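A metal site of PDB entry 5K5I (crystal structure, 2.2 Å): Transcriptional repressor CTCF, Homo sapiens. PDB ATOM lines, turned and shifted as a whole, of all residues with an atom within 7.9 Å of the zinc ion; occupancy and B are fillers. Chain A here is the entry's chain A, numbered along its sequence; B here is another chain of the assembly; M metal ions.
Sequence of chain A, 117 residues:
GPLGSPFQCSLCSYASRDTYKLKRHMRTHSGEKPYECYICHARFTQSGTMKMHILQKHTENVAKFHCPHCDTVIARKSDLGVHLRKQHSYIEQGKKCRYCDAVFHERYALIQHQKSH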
ATOM      1  N   HIS A  66       9.077   3.501 -22.253  1.00  0.00           N
ATOM      2  CA  HIS A  66      10.359   4.195 -22.269  1.00  0.00           C
ATOM      3  C   HIS A  66      11.229   3.709 -21.123  1.00  0.00           C
ATOM      4  O   HIS A  66      10.759   3.518 -20.005  1.00  0.00           O
ATOM      5  CB  HIS A  66      10.142   5.714 -22.160  1.00  0.00           C
ATOM      6  CG  HIS A  66      11.382   6.519 -22.378  1.00  0.00           C
ATOM      7  ND1 HIS A  66      12.298   6.766 -21.377  1.00  0.00           N
ATOM      8  CD2 HIS A  66      11.857   7.145 -23.483  1.00  0.00           C
ATOM      9  CE1 HIS A  66      13.281   7.501 -21.856  1.00  0.00           C
ATOM     10  NE2 HIS A  66      13.037   7.747 -23.129  1.00  0.00           N
ATOM     11  N   CYS A  67      12.510   3.490 -21.427  1.00  0.00           N
ATOM     12  CA  CYS A  67      13.434   3.003 -20.411  1.00  0.00           C
ATOM     13  C   CYS A  67      13.801   4.117 -19.432  1.00  0.00           C
ATOM     14  O   CYS A  67      13.984   5.275 -19.844  1.00  0.00           O
ATOM     15  CB  CYS A  67      14.710   2.456 -21.061  1.00  0.00           C
ATOM     16  SG  CYS A  67      15.938   1.849 -19.877  1.00  0.00           S
ATOM     17  N   PRO A  68      13.889   3.819 -18.135  1.00  0.00           N
ATOM     18  CA  PRO A  68      14.232   4.863 -17.155  1.00  0.00           C
ATOM     19  C   PRO A  68      15.711   5.222 -17.105  1.00  0.00           C
ATOM     20  O   PRO A  68      16.044   6.321 -16.648  1.00  0.00           O
ATOM     21  CB  PRO A  68      13.772   4.262 -15.822  1.00  0.00           C
ATOM     22  CG  PRO A  68      13.865   2.789 -16.038  1.00  0.00           C
ATOM     23  CD  PRO A  68      13.504   2.563 -17.477  1.00  0.00           C
ATOM     24  N   HIS A  69      16.607   4.337 -17.544  1.00  0.00           N
ATOM     25  CA  HIS A  69      18.040   4.588 -17.444  1.00  0.00           C
ATOM     26  C   HIS A  69      18.667   5.044 -18.754  1.00  0.00           C
ATOM     27  O   HIS A  69      19.867   5.363 -18.772  1.00  0.00           O
ATOM     28  CB  HIS A  69      18.763   3.320 -16.951  1.00  0.00           C
ATOM     29  CG  HIS A  69      20.024   3.602 -16.184  1.00  0.00           C
ATOM     30  ND1 HIS A  69      20.068   4.460 -15.107  1.00  0.00           N
ATOM     31  CD2 HIS A  69      21.279   3.111 -16.332  1.00  0.00           C
ATOM     32  CE1 HIS A  69      21.305   4.493 -14.634  1.00  0.00           C
ATOM     33  NE2 HIS A  69      22.054   3.692 -15.353  1.00  0.00           N
ATOM     34  N   CYS A  70      17.903   5.104 -19.838  1.00  0.00           N
ATOM     35  CA  CYS A  70      18.406   5.621 -21.107  1.00  0.00           C
ATOM     36  C   CYS A  70      17.221   6.148 -21.917  1.00  0.00           C
ATOM     37  O   CYS A  70      16.118   6.333 -21.380  1.00  0.00           O
ATOM     38  CB  CYS A  70      19.182   4.538 -21.867  1.00  0.00           C
ATOM     39  SG  CYS A  70      18.173   3.248 -22.628  1.00  0.00           S
ATOM     40  N   ASP A  71      17.448   6.401 -23.198  1.00  0.00           N
ATOM     41  CA  ASP A  71      16.438   6.974 -24.076  1.00  0.00           C
ATOM     42  C   ASP A  71      15.782   5.952 -25.004  1.00  0.00           C
ATOM     43  O   ASP A  71      15.027   6.339 -25.894  1.00  0.00           O
ATOM     44  CB  ASP A  71      17.037   8.116 -24.905  1.00  0.00           C
ATOM     45  CG  ASP A  71      17.513   9.265 -24.040  1.00  0.00           C
ATOM     46  OD1 ASP A  71      16.951   9.467 -22.953  1.00  0.00           O
ATOM     47  OD2 ASP A  71      18.455   9.977 -24.467  1.00  0.00           O
ATOM     48  N   THR A  72      16.057   4.671 -24.820  1.00  0.00           N
ATOM     49  CA  THR A  72      15.501   3.650 -25.704  1.00  0.00           C
ATOM     50  C   THR A  72      14.017   3.457 -25.411  1.00  0.00           C
ATOM     51  O   THR A  72      13.593   3.350 -24.262  1.00  0.00           O
ATOM     52  CB  THR A  72      16.238   2.333 -25.530  1.00  0.00           C
ATOM     53  OG1 THR A  72      17.640   2.539 -25.749  1.00  0.00           O
ATOM     54  CG2 THR A  72      15.725   1.292 -26.518  1.00  0.00           C
ATOM     55  N   VAL A  73      13.217   3.408 -26.481  1.00  0.00           N
ATOM     56  CA  VAL A  73      11.786   3.132 -26.391  1.00  0.00           C
ATOM     57  C   VAL A  73      11.548   1.723 -26.908  1.00  0.00           C
ATOM     58  O   VAL A  73      12.155   1.292 -27.895  1.00  0.00           O
ATOM     59  CB  VAL A  73      10.958   4.168 -27.176  1.00  0.00           C
ATOM     60  CG1 VAL A  73      11.393   4.235 -28.643  1.00  0.00           C
ATOM     61  CG2 VAL A  73       9.466   3.871 -27.069  1.00  0.00           C
ATOM     62  N   ILE A  74      10.677   0.982 -26.219  1.00  0.00           N
ATOM     63  CA  ILE A  74      10.400  -0.416 -26.526  1.00  0.00           C
ATOM     64  C   ILE A  74       8.901  -0.641 -26.528  1.00  0.00           C
ATOM     65  O   ILE A  74       8.183  -0.078 -25.682  1.00  0.00           O
ATOM     66  CB  ILE A  74      11.098  -1.363 -25.523  1.00  0.00           C
ATOM     67  CG1 ILE A  74      12.608  -1.187 -25.581  1.00  0.00           C
ATOM     68  CG2 ILE A  74      10.735  -2.806 -25.789  1.00  0.00           C
ATOM     69  CD1 ILE A  74      13.359  -2.076 -24.631  1.00  0.00           C
ATOM     70  N   LEU A  80      11.146  -4.680 -22.434  1.00  0.00           N
ATOM     71  CA  LEU A  80      11.841  -3.685 -21.633  1.00  0.00           C
ATOM     72  C   LEU A  80      12.553  -4.345 -20.451  1.00  0.00           C
ATOM     73  O   LEU A  80      13.641  -3.917 -20.054  1.00  0.00           O
ATOM     74  CB  LEU A  80      10.867  -2.620 -21.153  1.00  0.00           C
ATOM     75  CG  LEU A  80      11.442  -1.549 -20.223  1.00  0.00           C
ATOM     76  CD1 LEU A  80      12.593  -0.813 -20.881  1.00  0.00           C
ATOM     77  CD2 LEU A  80      10.358  -0.573 -19.783  1.00  0.00           C
ATOM     78  N   HIS A  83      15.687  -5.596 -21.711  1.00  0.00           N
ATOM     79  CA  HIS A  83      16.612  -4.481 -21.886  1.00  0.00           C
ATOM     80  C   HIS A  83      17.247  -4.084 -20.562  1.00  0.00           C
ATOM     81  O   HIS A  83      18.461  -3.888 -20.475  1.00  0.00           O
ATOM     82  CB  HIS A  83      15.878  -3.298 -22.511  1.00  0.00           C
ATOM     83  CG  HIS A  83      16.709  -2.053 -22.625  1.00  0.00           C
ATOM     84  ND1 HIS A  83      17.523  -1.806 -23.707  1.00  0.00           N
ATOM     85  CD2 HIS A  83      16.846  -1.001 -21.797  1.00  0.00           C
ATOM     86  CE1 HIS A  83      18.129  -0.641 -23.544  1.00  0.00           C
ATOM     87  NE2 HIS A  83      17.733  -0.135 -22.390  1.00  0.00           N
ATOM     88  N   LEU A  84      16.433  -3.942 -19.511  1.00  0.00           N
ATOM     89  CA  LEU A  84      16.945  -3.547 -18.211  1.00  0.00           C
ATOM     90  C   LEU A  84      17.933  -4.572 -17.667  1.00  0.00           C
ATOM     91  O   LEU A  84      18.978  -4.209 -17.117  1.00  0.00           O
ATOM     92  CB  LEU A  84      15.796  -3.334 -17.229  1.00  0.00           C
ATOM     93  CG  LEU A  84      14.880  -2.137 -17.501  1.00  0.00           C
ATOM     94  CD1 LEU A  84      13.662  -2.175 -16.598  1.00  0.00           C
ATOM     95  CD2 LEU A  84      15.634  -0.821 -17.335  1.00  0.00           C
ATOM     96  N   GLN A  87      21.139  -4.617 -20.432  1.00  0.00           N
ATOM     97  CA  GLN A  87      21.889  -3.393 -20.674  1.00  0.00           C
ATOM     98  C   GLN A  87      22.259  -2.630 -19.411  1.00  0.00           C
ATOM     99  O   GLN A  87      23.351  -2.067 -19.325  1.00  0.00           O
ATOM    100  CB  GLN A  87      21.098  -2.448 -21.592  1.00  0.00           C
ATOM    101  CG  GLN A  87      20.655  -3.074 -22.909  1.00  0.00           C
ATOM    102  CD  GLN A  87      21.831  -3.479 -23.791  1.00  0.00           C
ATOM    103  OE1 GLN A  87      22.910  -2.897 -23.709  1.00  0.00           O
ATOM    104  NE2 GLN A  87      21.613  -4.479 -24.631  1.00  0.00           N
ATOM    105  N   HIS A  88      21.369  -2.596 -18.419  1.00  0.00           N
ATOM    106  CA  HIS A  88      21.566  -1.751 -17.249  1.00  0.00           C
ATOM    107  C   HIS A  88      21.834  -2.534 -15.966  1.00  0.00           C
ATOM    108  O   HIS A  88      21.791  -1.959 -14.880  1.00  0.00           O
ATOM    109  CB  HIS A  88      20.356  -0.819 -17.056  1.00  0.00           C
ATOM    110  CG  HIS A  88      20.082   0.059 -18.234  1.00  0.00           C
ATOM    111  ND1 HIS A  88      20.988   0.980 -18.700  1.00  0.00           N
ATOM    112  CD2 HIS A  88      18.995   0.147 -19.042  1.00  0.00           C
ATOM    113  CE1 HIS A  88      20.478   1.601 -19.750  1.00  0.00           C
ATOM    114  NE2 HIS A  88      19.276   1.116 -19.973  1.00  0.00           N
ATOM    115  N   TYR A 108      25.182  -0.801 -21.429  1.00  0.00           N
ATOM    116  CA  TYR A 108      24.714   0.207 -22.374  1.00  0.00           C
ATOM    117  C   TYR A 108      25.704   1.365 -22.504  1.00  0.00           C
ATOM    118  O   TYR A 108      25.984   1.827 -23.621  1.00  0.00           O
ATOM    119  CB  TYR A 108      23.337   0.724 -21.955  1.00  0.00           C
ATOM    120  CG  TYR A 108      22.694   1.640 -22.978  1.00  0.00           C
ATOM    121  CD1 TYR A 108      21.982   1.117 -24.046  1.00  0.00           C
ATOM    122  CD2 TYR A 108      22.814   3.019 -22.879  1.00  0.00           C
ATOM    123  CE1 TYR A 108      21.389   1.946 -24.985  1.00  0.00           C
ATOM    124  CE2 TYR A 108      22.224   3.861 -23.822  1.00  0.00           C
ATOM    125  CZ  TYR A 108      21.518   3.314 -24.866  1.00  0.00           C
ATOM    126  OH  TYR A 108      20.934   4.134 -25.799  1.00  0.00           O
ATOM    127  P    DG B   3      17.099  -3.714 -26.948  1.00  0.00           P
ATOM    128  OP1  DG B   3      17.539  -2.472 -26.288  1.00  0.00           O
ATOM    129  OP2  DG B   3      16.975  -4.960 -26.149  1.00  0.00           O
ATOM    130  O5'  DG B   3      15.690  -3.454 -27.667  1.00  0.00           O
ATOM    131  C5'  DG B   3      15.578  -2.401 -28.615  1.00  0.00           C
ATOM    132  C4'  DG B   3      14.744  -2.830 -29.810  1.00  0.00           C
ATOM    133  O4'  DG B   3      15.311  -4.021 -30.399  1.00  0.00           O
ATOM    134  C3'  DG B   3      13.286  -3.167 -29.502  1.00  0.00           C
ATOM    135  O3'  DG B   3      12.450  -2.739 -30.565  1.00  0.00           O
ATOM    136  C2'  DG B   3      13.303  -4.686 -29.375  1.00  0.00           C
ATOM    137  C1'  DG B   3      14.373  -5.076 -30.392  1.00  0.00           C
ATOM    138  N9   DG B   3      15.080  -6.308 -30.050  1.00  0.00           N
ATOM    139  C8   DG B   3      15.713  -6.597 -28.869  1.00  0.00           C
ATOM    140  N7   DG B   3      16.274  -7.779 -28.857  1.00  0.00           N
ATOM    141  C5   DG B   3      15.995  -8.304 -30.102  1.00  0.00           C
ATOM    142  C6   DG B   3      16.349  -9.554 -30.668  1.00  0.00           C
ATOM    143  O6   DG B   3      16.996 -10.466 -30.149  1.00  0.00           O
ATOM    144  N1   DG B   3      15.870  -9.684 -31.967  1.00  0.00           N
ATOM    145  C2   DG B   3      15.135  -8.737 -32.639  1.00  0.00           C
ATOM    146  N2   DG B   3      14.757  -9.046 -33.893  1.00  0.00           N
ATOM    147  N3   DG B   3      14.798  -7.557 -32.122  1.00  0.00           N
ATOM    148  C4   DG B   3      15.261  -7.414 -30.864  1.00  0.00           C
HETATM  149 ZN    ZN M   1      17.725   1.526 -21.198  1.00  0.00          ZN
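NE2 of His 88 is bound to the zinc ion, 2.0 Å away.
NE2 of His 83 binds the zinc ion, at 2.0 Å.
SG of Cys 67 is bound to the zinc ion.
The zinc ion is bound by the side-chain sulfur (SG) of Cys 70 (2.3 Å).
The zinc ion has four donor atoms within binding distance.
Of the 16 residues printed, 4 come within 4 Å of the zinc ion.
A ring nitrogen (ND1) of His 83 lies within hydrogen-bond range of OP1 of DG 3 of chain B, 2.7 Å away.
N of His 69 lies close to SG of Cys 67 (3.5 Å).
O of Thr 72 sits at hydrogen-bond distance from N of Cys 67.
OG1 of Thr 72 sits close to SG of Cys 70.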
